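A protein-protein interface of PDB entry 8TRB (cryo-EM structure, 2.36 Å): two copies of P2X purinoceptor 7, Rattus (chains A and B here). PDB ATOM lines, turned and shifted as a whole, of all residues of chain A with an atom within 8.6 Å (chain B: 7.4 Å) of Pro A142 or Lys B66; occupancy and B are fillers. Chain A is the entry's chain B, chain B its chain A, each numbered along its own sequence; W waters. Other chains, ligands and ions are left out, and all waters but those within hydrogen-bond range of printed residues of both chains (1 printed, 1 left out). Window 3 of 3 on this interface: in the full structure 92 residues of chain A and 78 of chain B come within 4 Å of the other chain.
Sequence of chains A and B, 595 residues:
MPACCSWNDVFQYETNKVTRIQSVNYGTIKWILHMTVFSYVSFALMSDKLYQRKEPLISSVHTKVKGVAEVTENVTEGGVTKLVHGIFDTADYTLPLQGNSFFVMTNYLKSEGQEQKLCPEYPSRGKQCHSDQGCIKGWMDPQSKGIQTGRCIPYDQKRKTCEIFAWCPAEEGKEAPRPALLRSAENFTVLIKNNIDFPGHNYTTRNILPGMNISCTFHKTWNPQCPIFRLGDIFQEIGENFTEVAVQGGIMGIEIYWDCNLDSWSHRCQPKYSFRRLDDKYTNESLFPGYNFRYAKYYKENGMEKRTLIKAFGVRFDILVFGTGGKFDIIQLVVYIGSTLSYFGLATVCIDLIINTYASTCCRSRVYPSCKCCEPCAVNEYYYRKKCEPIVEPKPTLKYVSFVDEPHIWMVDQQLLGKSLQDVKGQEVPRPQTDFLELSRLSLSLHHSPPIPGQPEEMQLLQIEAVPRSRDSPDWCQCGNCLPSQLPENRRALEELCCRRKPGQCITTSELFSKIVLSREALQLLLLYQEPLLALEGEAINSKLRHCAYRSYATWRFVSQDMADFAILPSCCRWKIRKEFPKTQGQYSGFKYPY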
ATOM      1  N   GLU A 121      -3.267  10.425  22.496  1.00  0.00           N
ATOM      2  CA  GLU A 121      -2.117  11.289  22.305  1.00  0.00           C
ATOM      3  C   GLU A 121      -1.878  12.139  23.547  1.00  0.00           C
ATOM      4  O   GLU A 121      -2.809  12.508  24.266  1.00  0.00           O
ATOM      5  CB  GLU A 121      -2.314  12.170  21.069  1.00  0.00           C
ATOM      6  CG  GLU A 121      -3.107  13.432  21.292  1.00  0.00           C
ATOM      7  CD  GLU A 121      -3.595  14.045  19.995  1.00  0.00           C
ATOM      8  OE1 GLU A 121      -3.012  13.744  18.935  1.00  0.00           O
ATOM      9  OE2 GLU A 121      -4.566  14.829  20.037  1.00  0.00           O
ATOM     10  N   LYS A 127      -3.870  20.174  24.383  1.00  0.00           N
ATOM     11  CA  LYS A 127      -4.417  19.436  23.244  1.00  0.00           C
ATOM     12  C   LYS A 127      -5.521  18.487  23.713  1.00  0.00           C
ATOM     13  O   LYS A 127      -5.481  17.274  23.507  1.00  0.00           O
ATOM     14  CB  LYS A 127      -3.311  18.679  22.523  1.00  0.00           C
ATOM     15  CG  LYS A 127      -3.724  18.120  21.187  1.00  0.00           C
ATOM     16  CD  LYS A 127      -2.522  17.611  20.421  1.00  0.00           C
ATOM     17  CE  LYS A 127      -2.118  18.564  19.312  1.00  0.00           C
ATOM     18  NZ  LYS A 127      -0.711  18.351  18.879  1.00  0.00           N
ATOM     19  N   TRP A 139      -6.075  11.358  10.050  1.00  0.00           N
ATOM     20  CA  TRP A 139      -5.193  12.513  10.034  1.00  0.00           C
ATOM     21  C   TRP A 139      -3.848  12.151  10.649  1.00  0.00           C
ATOM     22  O   TRP A 139      -3.785  11.655  11.778  1.00  0.00           O
ATOM     23  CB  TRP A 139      -5.837  13.676  10.778  1.00  0.00           C
ATOM     24  CG  TRP A 139      -5.040  14.930  10.718  1.00  0.00           C
ATOM     25  CD1 TRP A 139      -4.668  15.612   9.600  1.00  0.00           C
ATOM     26  CD2 TRP A 139      -4.513  15.661  11.829  1.00  0.00           C
ATOM     27  NE1 TRP A 139      -3.936  16.721   9.945  1.00  0.00           N
ATOM     28  CE2 TRP A 139      -3.828  16.774  11.309  1.00  0.00           C
ATOM     29  CE3 TRP A 139      -4.551  15.482  13.212  1.00  0.00           C
ATOM     30  CZ2 TRP A 139      -3.188  17.702  12.123  1.00  0.00           C
ATOM     31  CZ3 TRP A 139      -3.920  16.403  14.018  1.00  0.00           C
ATOM     32  CH2 TRP A 139      -3.245  17.499  13.473  1.00  0.00           C
ATOM     33  N   MET A 140      -2.759  12.403   9.925  1.00  0.00           N
ATOM     34  CA  MET A 140      -1.395  12.101  10.421  1.00  0.00           C
ATOM     35  C   MET A 140      -0.872  13.350  11.129  1.00  0.00           C
ATOM     36  O   MET A 140      -0.516  14.298  10.422  1.00  0.00           O
ATOM     37  CB  MET A 140      -0.473  11.682   9.271  1.00  0.00           C
ATOM     38  CG  MET A 140      -1.072  10.570   8.429  1.00  0.00           C
ATOM     39  SD  MET A 140       0.153   9.517   7.609  1.00  0.00           S
ATOM     40  CE  MET A 140       0.660  10.594   6.271  1.00  0.00           C
ATOM     41  N   ASP A 141      -0.881  13.363  12.463  1.00  0.00           N
ATOM     42  CA  ASP A 141      -0.388  14.469  13.261  1.00  0.00           C
ATOM     43  C   ASP A 141       1.121  14.345  13.391  1.00  0.00           C
ATOM     44  O   ASP A 141       1.597  13.424  14.069  1.00  0.00           O
ATOM     45  CB  ASP A 141      -1.035  14.477  14.633  1.00  0.00           C
ATOM     46  CG  ASP A 141      -0.805  15.775  15.378  1.00  0.00           C
ATOM     47  OD1 ASP A 141       0.146  16.502  15.024  1.00  0.00           O
ATOM     48  OD2 ASP A 141      -1.573  16.074  16.314  1.00  0.00           O
ATOM     49  N   PRO A 142       1.910  15.217  12.757  1.00  0.00           N
ATOM     50  CA  PRO A 142       3.365  15.124  12.913  1.00  0.00           C
ATOM     51  C   PRO A 142       3.847  15.522  14.294  1.00  0.00           C
ATOM     52  O   PRO A 142       4.983  15.185  14.652  1.00  0.00           O
ATOM     53  CB  PRO A 142       3.898  16.077  11.827  1.00  0.00           C
ATOM     54  CG  PRO A 142       2.734  16.363  10.945  1.00  0.00           C
ATOM     55  CD  PRO A 142       1.544  16.297  11.830  1.00  0.00           C
ATOM     56  N   GLN A 143       3.026  16.224  15.075  1.00  0.00           N
ATOM     57  CA  GLN A 143       3.374  16.521  16.458  1.00  0.00           C
ATOM     58  C   GLN A 143       3.159  15.303  17.348  1.00  0.00           C
ATOM     59  O   GLN A 143       4.051  14.912  18.108  1.00  0.00           O
ATOM     60  CB  GLN A 143       2.550  17.705  16.965  1.00  0.00           C
ATOM     61  N   SER A 144       1.978  14.695  17.265  1.00  0.00           N
ATOM     62  CA  SER A 144       1.695  13.488  18.027  1.00  0.00           C
ATOM     63  C   SER A 144       2.415  12.272  17.467  1.00  0.00           C
ATOM     64  O   SER A 144       2.673  11.323  18.214  1.00  0.00           O
ATOM     65  CB  SER A 144       0.193  13.228  18.051  1.00  0.00           C
ATOM     66  OG  SER A 144      -0.180  12.341  17.014  1.00  0.00           O
ATOM     67  N   LYS A 145       2.734  12.282  16.175  1.00  0.00           N
ATOM     68  CA  LYS A 145       3.468  11.198  15.531  1.00  0.00           C
ATOM     69  C   LYS A 145       2.625   9.928  15.469  1.00  0.00           C
ATOM     70  O   LYS A 145       3.090   8.824  15.751  1.00  0.00           O
ATOM     71  CB  LYS A 145       4.801  10.955  16.239  1.00  0.00           C
ATOM     72  CG  LYS A 145       5.621  12.200  16.386  1.00  0.00           C
ATOM     73  CD  LYS A 145       7.063  11.949  16.105  1.00  0.00           C
ATOM     74  CE  LYS A 145       7.853  13.233  16.070  1.00  0.00           C
ATOM     75  NZ  LYS A 145       7.501  14.137  17.170  1.00  0.00           N
ATOM     76  N   GLY A 146       1.367  10.098  15.076  1.00  0.00           N
ATOM     77  CA  GLY A 146       0.442   8.990  14.943  1.00  0.00           C
ATOM     78  C   GLY A 146      -0.720   9.363  14.054  1.00  0.00           C
ATOM     79  O   GLY A 146      -0.913  10.524  13.690  1.00  0.00           O
ATOM     80  N   ILE A 147      -1.500   8.344  13.707  1.00  0.00           N
ATOM     81  CA  ILE A 147      -2.667   8.487  12.846  1.00  0.00           C
ATOM     82  C   ILE A 147      -3.909   8.543  13.720  1.00  0.00           C
ATOM     83  O   ILE A 147      -4.218   7.584  14.433  1.00  0.00           O
ATOM     84  CB  ILE A 147      -2.776   7.329  11.844  1.00  0.00           C
ATOM     85  CG1 ILE A 147      -1.404   6.890  11.346  1.00  0.00           C
ATOM     86  CG2 ILE A 147      -3.647   7.735  10.676  1.00  0.00           C
ATOM     87  CD1 ILE A 147      -0.602   7.970  10.728  1.00  0.00           C
ATOM     88  N   GLN A 148      -4.636   9.652  13.646  1.00  0.00           N
ATOM     89  CA  GLN A 148      -5.885   9.774  14.381  1.00  0.00           C
ATOM     90  C   GLN A 148      -6.933   8.809  13.842  1.00  0.00           C
ATOM     91  O   GLN A 148      -7.014   8.545  12.641  1.00  0.00           O
ATOM     92  CB  GLN A 148      -6.419  11.198  14.307  1.00  0.00           C
ATOM     93  CG  GLN A 148      -5.603  12.221  15.054  1.00  0.00           C
ATOM     94  CD  GLN A 148      -6.344  13.516  15.244  1.00  0.00           C
ATOM     95  OE1 GLN A 148      -7.221  13.862  14.457  1.00  0.00           O
ATOM     96  NE2 GLN A 148      -5.996  14.246  16.293  1.00  0.00           N
ATOM     97  N   GLU A 172       4.867  12.196  23.203  1.00  0.00           N
ATOM     98  CA  GLU A 172       5.342  13.354  22.462  1.00  0.00           C
ATOM     99  C   GLU A 172       4.580  14.607  22.869  1.00  0.00           C
ATOM    100  O   GLU A 172       3.351  14.603  22.978  1.00  0.00           O
ATOM    101  CB  GLU A 172       5.200  13.113  20.962  1.00  0.00           C
ATOM    102  CG  GLU A 172       6.135  12.057  20.411  1.00  0.00           C
ATOM    103  CD  GLU A 172       7.599  12.399  20.624  1.00  0.00           C
ATOM    104  OE1 GLU A 172       8.026  13.496  20.212  1.00  0.00           O
ATOM    105  OE2 GLU A 172       8.324  11.569  21.212  1.00  0.00           O
ATOM    106  N   GLY A 173       5.320  15.690  23.070  1.00  0.00           N
ATOM    107  CA  GLY A 173       4.786  16.912  23.621  1.00  0.00           C
ATOM    108  C   GLY A 173       5.070  17.104  25.089  1.00  0.00           C
ATOM    109  O   GLY A 173       4.878  18.211  25.603  1.00  0.00           O
ATOM    110  N   GLU A 285       8.256  28.657  19.797  1.00  0.00           N
ATOM    111  CA  GLU A 285       7.961  27.305  20.260  1.00  0.00           C
ATOM    112  C   GLU A 285       7.510  26.410  19.118  1.00  0.00           C
ATOM    113  O   GLU A 285       7.740  25.196  19.150  1.00  0.00           O
ATOM    114  CB  GLU A 285       6.892  27.346  21.350  1.00  0.00           C
ATOM    115  N   SER A 286       6.864  26.985  18.108  1.00  0.00           N
ATOM    116  CA  SER A 286       6.448  26.215  16.947  1.00  0.00           C
ATOM    117  C   SER A 286       7.623  25.798  16.078  1.00  0.00           C
ATOM    118  O   SER A 286       7.494  24.852  15.295  1.00  0.00           O
ATOM    119  CB  SER A 286       5.457  27.028  16.124  1.00  0.00           C
ATOM    120  OG  SER A 286       6.130  27.981  15.324  1.00  0.00           O
ATOM    121  N   LEU A 287       8.764  26.473  16.200  1.00  0.00           N
ATOM    122  CA  LEU A 287       9.921  26.214  15.356  1.00  0.00           C
ATOM    123  C   LEU A 287      10.960  25.331  16.033  1.00  0.00           C
ATOM    124  O   LEU A 287      12.136  25.383  15.661  1.00  0.00           O
ATOM    125  CB  LEU A 287      10.557  27.534  14.927  1.00  0.00           C
ATOM    126  CG  LEU A 287       9.782  28.388  13.931  1.00  0.00           C
ATOM    127  CD1 LEU A 287      10.554  29.651  13.651  1.00  0.00           C
ATOM    128  CD2 LEU A 287       9.522  27.625  12.652  1.00  0.00           C
ATOM    129  N   PHE A 288      10.556  24.535  17.012  1.00  0.00           N
ATOM    130  CA  PHE A 288      11.419  23.544  17.640  1.00  0.00           C
ATOM    131  C   PHE A 288      12.645  24.203  18.257  1.00  0.00           C
ATOM    132  O   PHE A 288      13.762  24.070  17.744  1.00  0.00           O
ATOM    133  CB  PHE A 288      11.803  22.477  16.622  1.00  0.00           C
ATOM    134  CG  PHE A 288      10.645  21.996  15.814  1.00  0.00           C
ATOM    135  CD1 PHE A 288       9.469  21.616  16.437  1.00  0.00           C
ATOM    136  CD2 PHE A 288      10.718  21.938  14.438  1.00  0.00           C
ATOM    137  CE1 PHE A 288       8.393  21.184  15.703  1.00  0.00           C
ATOM    138  CE2 PHE A 288       9.647  21.503  13.702  1.00  0.00           C
ATOM    139  CZ  PHE A 288       8.483  21.125  14.334  1.00  0.00           C
ATOM    140  N   ARG A 294      15.297  12.249  18.435  1.00  0.00           N
ATOM    141  CA  ARG A 294      14.645  11.052  18.954  1.00  0.00           C
ATOM    142  C   ARG A 294      15.414   9.823  18.492  1.00  0.00           C
ATOM    143  O   ARG A 294      15.639   9.640  17.290  1.00  0.00           O
ATOM    144  CB  ARG A 294      13.190  10.989  18.489  1.00  0.00           C
ATOM    145  CG  ARG A 294      12.313  12.078  19.082  1.00  0.00           C
ATOM    146  CD  ARG A 294      11.040  12.282  18.281  1.00  0.00           C
ATOM    147  NE  ARG A 294       9.988  11.355  18.688  1.00  0.00           N
ATOM    148  CZ  ARG A 294       9.598  10.293  17.995  1.00  0.00           C
ATOM    149  NH1 ARG A 294      10.155   9.974  16.839  1.00  0.00           N
ATOM    150  NH2 ARG A 294       8.623   9.529  18.477  1.00  0.00           N
ATOM    151  N   LYS B  64      15.062  19.620  10.828  1.00  0.00           N
ATOM    152  CA  LYS B  64      14.035  18.858  11.521  1.00  0.00           C
ATOM    153  C   LYS B  64      13.021  18.343  10.513  1.00  0.00           C
ATOM    154  O   LYS B  64      12.377  19.130   9.820  1.00  0.00           O
ATOM    155  CB  LYS B  64      13.338  19.700  12.593  1.00  0.00           C
ATOM    156  CG  LYS B  64      12.379  18.927  13.475  1.00  0.00           C
ATOM    157  CD  LYS B  64      13.078  17.886  14.326  1.00  0.00           C
ATOM    158  CE  LYS B  64      14.141  18.495  15.229  1.00  0.00           C
ATOM    159  NZ  LYS B  64      14.429  17.629  16.389  1.00  0.00           N
ATOM    160  N   VAL B  65      12.877  17.025  10.445  1.00  0.00           N
ATOM    161  CA  VAL B  65      11.911  16.373   9.570  1.00  0.00           C
ATOM    162  C   VAL B  65      10.639  16.101  10.356  1.00  0.00           C
ATOM    163  O   VAL B  65      10.683  15.600  11.485  1.00  0.00           O
ATOM    164  CB  VAL B  65      12.483  15.075   8.971  1.00  0.00           C
ATOM    165  CG1 VAL B  65      11.460  14.378   8.082  1.00  0.00           C
ATOM    166  CG2 VAL B  65      13.738  15.368   8.189  1.00  0.00           C
ATOM    167  N   LYS B  66       9.508  16.459   9.763  1.00  0.00           N
ATOM    168  CA  LYS B  66       8.182  16.168  10.279  1.00  0.00           C
ATOM    169  C   LYS B  66       7.451  15.265   9.299  1.00  0.00           C
ATOM    170  O   LYS B  66       7.531  15.458   8.080  1.00  0.00           O
ATOM    171  CB  LYS B  66       7.366  17.447  10.505  1.00  0.00           C
ATOM    172  CG  LYS B  66       7.943  18.405  11.516  1.00  0.00           C
ATOM    173  CD  LYS B  66       7.302  19.778  11.412  1.00  0.00           C
ATOM    174  CE  LYS B  66       5.993  19.864  12.161  1.00  0.00           C
ATOM    175  NZ  LYS B  66       5.540  21.274  12.298  1.00  0.00           N
ATOM    176  N   GLY B  67       6.745  14.291   9.834  1.00  0.00           N
ATOM    177  CA  GLY B  67       5.920  13.403   9.044  1.00  0.00           C
ATOM    178  C   GLY B  67       5.841  12.004   9.613  1.00  0.00           C
ATOM    179  O   GLY B  67       6.742  11.506  10.272  1.00  0.00           O
ATOM    180  N   VAL B  68       4.716  11.349   9.343  1.00  0.00           N
ATOM    181  CA  VAL B  68       4.476   9.961   9.706  1.00  0.00           C
ATOM    182  C   VAL B  68       4.052   9.224   8.447  1.00  0.00           C
ATOM    183  O   VAL B  68       3.265   9.749   7.654  1.00  0.00           O
ATOM    184  CB  VAL B  68       3.396   9.813  10.798  1.00  0.00           C
ATOM    185  CG1 VAL B  68       3.422   8.424  11.386  1.00  0.00           C
ATOM    186  CG2 VAL B  68       3.577  10.824  11.888  1.00  0.00           C
ATOM    187  N   ASP B  89       7.511   6.863  12.369  1.00  0.00           N
ATOM    188  CA  ASP B  89       7.788   8.236  12.742  1.00  0.00           C
ATOM    189  C   ASP B  89       9.273   8.526  12.538  1.00  0.00           C
ATOM    190  O   ASP B  89      10.049   7.671  12.110  1.00  0.00           O
ATOM    191  CB  ASP B  89       7.324   8.526  14.175  1.00  0.00           C
ATOM    192  CG  ASP B  89       8.067   7.732  15.229  1.00  0.00           C
ATOM    193  OD1 ASP B  89       9.304   7.607  15.160  1.00  0.00           O
ATOM    194  OD2 ASP B  89       7.397   7.259  16.164  1.00  0.00           O
ATOM    195  N   THR B  90       9.665   9.763  12.842  1.00  0.00           N
ATOM    196  CA  THR B  90      11.006  10.235  12.521  1.00  0.00           C
ATOM    197  C   THR B  90      12.089   9.292  13.027  1.00  0.00           C
ATOM    198  O   THR B  90      13.086   9.057  12.335  1.00  0.00           O
ATOM    199  CB  THR B  90      11.207  11.642  13.083  1.00  0.00           C
ATOM    200  OG1 THR B  90      10.863  11.662  14.472  1.00  0.00           O
ATOM    201  CG2 THR B  90      10.351  12.635  12.333  1.00  0.00           C
ATOM    202  N   TYR B  93      12.525   6.347  10.491  1.00  0.00           N
ATOM    203  CA  TYR B  93      12.921   6.564   9.107  1.00  0.00           C
ATOM    204  C   TYR B  93      13.980   7.636   8.919  1.00  0.00           C
ATOM    205  O   TYR B  93      14.457   7.794   7.794  1.00  0.00           O
ATOM    206  CB  TYR B  93      11.695   6.917   8.244  1.00  0.00           C
ATOM    207  CG  TYR B  93      11.031   8.244   8.541  1.00  0.00           C
ATOM    208  CD1 TYR B  93      11.644   9.437   8.215  1.00  0.00           C
ATOM    209  CD2 TYR B  93       9.777   8.301   9.113  1.00  0.00           C
ATOM    210  CE1 TYR B  93      11.053  10.628   8.472  1.00  0.00           C
ATOM    211  CE2 TYR B  93       9.172   9.503   9.371  1.00  0.00           C
ATOM    212  CZ  TYR B  93       9.818  10.664   9.051  1.00  0.00           C
ATOM    213  OH  TYR B  93       9.229  11.870   9.300  1.00  0.00           O
ATOM    214  N   THR B  94      14.368   8.371   9.953  1.00  0.00           N
ATOM    215  CA  THR B  94      15.244   9.523   9.806  1.00  0.00           C
ATOM    216  C   THR B  94      16.587   9.230  10.451  1.00  0.00           C
ATOM    217  O   THR B  94      16.648   8.668  11.547  1.00  0.00           O
ATOM    218  CB  THR B  94      14.641  10.781  10.436  1.00  0.00           C
ATOM    219  OG1 THR B  94      13.372  11.056   9.852  1.00  0.00           O
ATOM    220  CG2 THR B  94      15.509  11.969  10.169  1.00  0.00           C
ATOM    221  N   ALA B 185       6.652   9.560   2.234  1.00  0.00           N
ATOM    222  CA  ALA B 185       7.720  10.488   2.568  1.00  0.00           C
ATOM    223  C   ALA B 185       7.739  11.705   1.656  1.00  0.00           C
ATOM    224  O   ALA B 185       8.301  12.735   2.036  1.00  0.00           O
ATOM    225  CB  ALA B 185       9.062   9.765   2.522  1.00  0.00           C
ATOM    226  N   ASN B 187       5.387  13.555   1.230  1.00  0.00           N
ATOM    227  CA  ASN B 187       4.601  14.514   1.975  1.00  0.00           C
ATOM    228  C   ASN B 187       5.268  14.954   3.270  1.00  0.00           C
ATOM    229  O   ASN B 187       4.741  15.842   3.945  1.00  0.00           O
ATOM    230  CB  ASN B 187       3.229  13.919   2.272  1.00  0.00           C
ATOM    231  CG  ASN B 187       2.276  14.038   1.111  1.00  0.00           C
ATOM    232  OD1 ASN B 187       2.335  14.986   0.336  1.00  0.00           O
ATOM    233  ND2 ASN B 187       1.388  13.068   0.988  1.00  0.00           N
ATOM    234  N   PHE B 188       6.411  14.373   3.623  1.00  0.00           N
ATOM    235  CA  PHE B 188       7.168  14.856   4.763  1.00  0.00           C
ATOM    236  C   PHE B 188       7.670  16.264   4.506  1.00  0.00           C
ATOM    237  O   PHE B 188       7.863  16.686   3.364  1.00  0.00           O
ATOM    238  CB  PHE B 188       8.369  13.958   5.062  1.00  0.00           C
ATOM    239  CG  PHE B 188       8.019  12.576   5.495  1.00  0.00           C
ATOM    240  CD1 PHE B 188       6.719  12.207   5.739  1.00  0.00           C
ATOM    241  CD2 PHE B 188       9.007  11.630   5.641  1.00  0.00           C
ATOM    242  CE1 PHE B 188       6.425  10.942   6.122  1.00  0.00           C
ATOM    243  CE2 PHE B 188       8.704  10.366   6.022  1.00  0.00           C
ATOM    244  CZ  PHE B 188       7.414  10.024   6.265  1.00  0.00           C
ATOM    245  N   THR B 189       7.887  16.992   5.589  1.00  0.00           N
ATOM    246  CA  THR B 189       8.449  18.327   5.525  1.00  0.00           C
ATOM    247  C   THR B 189       9.770  18.356   6.273  1.00  0.00           C
ATOM    248  O   THR B 189       9.995  17.578   7.198  1.00  0.00           O
ATOM    249  CB  THR B 189       7.499  19.371   6.113  1.00  0.00           C
ATOM    250  OG1 THR B 189       7.024  18.934   7.389  1.00  0.00           O
ATOM    251  CG2 THR B 189       6.327  19.602   5.195  1.00  0.00           C
ATOM    252  N   VAL B 190      10.656  19.236   5.839  1.00  0.00           N
ATOM    253  CA  VAL B 190      11.895  19.510   6.547  1.00  0.00           C
ATOM    254  C   VAL B 190      11.990  21.007   6.793  1.00  0.00           C
ATOM    255  O   VAL B 190      11.845  21.810   5.865  1.00  0.00           O
ATOM    256  CB  VAL B 190      13.136  18.991   5.791  1.00  0.00           C
ATOM    257  CG1 VAL B 190      13.327  19.697   4.459  1.00  0.00           C
ATOM    258  CG2 VAL B 190      14.372  19.113   6.663  1.00  0.00           C
ATOM    259  N   LEU B 191      12.203  21.372   8.046  1.00  0.00           N
ATOM    260  CA  LEU B 191      12.563  22.721   8.434  1.00  0.00           C
ATOM    261  C   LEU B 191      14.079  22.803   8.487  1.00  0.00           C
ATOM    262  O   LEU B 191      14.722  22.024   9.197  1.00  0.00           O
ATOM    263  CB  LEU B 191      11.943  23.083   9.779  1.00  0.00           C
ATOM    264  CG  LEU B 191      12.450  24.327  10.509  1.00  0.00           C
ATOM    265  CD1 LEU B 191      12.083  25.577   9.744  1.00  0.00           C
ATOM    266  CD2 LEU B 191      11.899  24.368  11.910  1.00  0.00           C
ATOM    267  N   ILE B 214       4.984  29.870  10.580  1.00  0.00           N
ATOM    268  CA  ILE B 214       5.255  28.441  10.467  1.00  0.00           C
ATOM    269  C   ILE B 214       4.313  27.776   9.480  1.00  0.00           C
ATOM    270  O   ILE B 214       4.640  26.718   8.932  1.00  0.00           O
ATOM    271  CB  ILE B 214       5.162  27.754  11.846  1.00  0.00           C
ATOM    272  CG1 ILE B 214       5.597  26.290  11.732  1.00  0.00           C
ATOM    273  CG2 ILE B 214       3.746  27.845  12.410  1.00  0.00           C
ATOM    274  CD1 ILE B 214       5.734  25.587  13.062  1.00  0.00           C
ATOM    275  N   ILE B 228      10.728  25.871   5.137  1.00  0.00           N
ATOM    276  CA  ILE B 228      10.034  24.603   5.301  1.00  0.00           C
ATOM    277  C   ILE B 228       9.773  24.039   3.916  1.00  0.00           C
ATOM    278  O   ILE B 228       9.088  24.665   3.099  1.00  0.00           O
ATOM    279  CB  ILE B 228       8.727  24.771   6.091  1.00  0.00           C
ATOM    280  CG1 ILE B 228       9.035  25.237   7.503  1.00  0.00           C
ATOM    281  CG2 ILE B 228       7.948  23.469   6.123  1.00  0.00           C
ATOM    282  CD1 ILE B 228       7.902  25.883   8.192  1.00  0.00           C
ATOM    283  N   PHE B 229      10.316  22.860   3.654  1.00  0.00           N
ATOM    284  CA  PHE B 229      10.302  22.256   2.335  1.00  0.00           C
ATOM    285  C   PHE B 229       9.618  20.902   2.386  1.00  0.00           C
ATOM    286  O   PHE B 229      10.020  20.029   3.156  1.00  0.00           O
ATOM    287  CB  PHE B 229      11.718  22.090   1.783  1.00  0.00           C
ATOM    288  CG  PHE B 229      12.552  23.325   1.850  1.00  0.00           C
ATOM    289  CD1 PHE B 229      13.220  23.664   3.003  1.00  0.00           C
ATOM    290  CD2 PHE B 229      12.686  24.137   0.749  1.00  0.00           C
ATOM    291  CE1 PHE B 229      13.986  24.792   3.053  1.00  0.00           C
ATOM    292  CE2 PHE B 229      13.452  25.259   0.804  1.00  0.00           C
ATOM    293  CZ  PHE B 229      14.099  25.587   1.952  1.00  0.00           C
ATOM    294  N   LEU B 231       9.328  17.435   0.665  1.00  0.00           N
ATOM    295  CA  LEU B 231      10.316  16.682  -0.099  1.00  0.00           C
ATOM    296  C   LEU B 231       9.860  16.465  -1.539  1.00  0.00           C
ATOM    297  O   LEU B 231      10.645  16.627  -2.486  1.00  0.00           O
ATOM    298  CB  LEU B 231      10.591  15.351   0.598  1.00  0.00           C
ATOM    299  CG  LEU B 231      10.843  15.409   2.106  1.00  0.00           C
ATOM    300  CD1 LEU B 231      11.298  14.064   2.631  1.00  0.00           C
ATOM    301  CD2 LEU B 231      11.834  16.492   2.492  1.00  0.00           C
HETATM  302  O   HOH W   1       7.026  14.299  12.910  1.00  0.00           O
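Water W1 lies within hydrogen-bond range of the backbone carbonyl oxygen (O) of Pro A142 (2.8 Å) and the backbone NH (N) of Gly B67 (3.1 Å).
Val B68 touches Asp A141 (CG2 to O, 3.9 Å).
Lys B66 touches Pro A142 (CB to CB, 3.96 Å).
N of Gly B67 touches CB of Pro A142 (3.9 Å).
Val B68 touches Lys A145 (CG2 to CA, 3.7 Å).
CD of Lys A145 touches CB of Asp B89, at 3.9 Å.
CE of Lys A145 touches OG1 of Thr B90, 3.8 Å away.
Lys B64 touches Phe A288 (CG to CD2, 3.6 Å).
Leu B191 touches Phe A288 (CD2 to CD2, 3.7 Å).
NH1 of Arg A294 lies within salt-bridge range of OD1 of Asp B89 (3.0 Å).
OG1 of Thr B90 is in hydrogen-bond range of NH1 of Arg A294, at 3.0 Å.
The side-chain sulfur of Met A140 sits close to the backbone carbonyl oxygen of Val B68 (3.1 Å).
No position is printed for both chains.
Of the 15 pairs that touch across the chains among the printed residues, none has its exchanged pair printed and touching as well.
Pro A142 touches just these residues of chain B: Lys B66 and Gly B67.
Of chain A, only Pro A142 (3.96 Å) and Phe A288 (3.4 Å) come within 4 Å of Lys B66.
Of chain A, only Pro A142 comes within 4 Å of Gly B67.
Of the printed residues of chain B, Ser A286 touches Ile B214 (2.9 Å).
Of the printed residues of chain B, Asp A141 touches Val B68.
Printed residues of chain B within 4 Å of Lys A145: Val B68, Asp B89 and Thr B90.
Ile A147 touches none of the printed residues of chain B.
The nearest residue of chain B that does not touch Pro A142 is Val B68 (4.4 Å).
The nearest residue of chain A that does not touch Lys B66 is Ser A286 (5.1 Å).
Of the 19 printed residues of chain A, 9 touch a printed residue of chain B.
Hydrophobic or aromatic side chains of chain A that line the printed part of chain B: Met A140, Pro A142 and Phe A288.
Of the 19 printed residues of chain B, 8 touch a printed residue of chain A.
Hydrophobic or aromatic side chains of chain B within 4 Å of the printed part of chain A: Val B68, Leu B191 and Ile B214.
Along chain B the printed residues that touch a printed residue of chain A span positions 64 to 214.
Among the printed residues, 15 pairs touch across the chains.
The backbone NH (N) of Leu B191 is in hydrogen-bond range of the backbone carbonyl oxygen (O) of Lys B64, 2.9 Å away.
OG of Ser A144 sits at hydrogen-bond distance from N of Gly A146 (3.3 Å).
NZ of Lys A145 is in salt-bridge range of OE1 of Glu A172 (3.2 Å).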
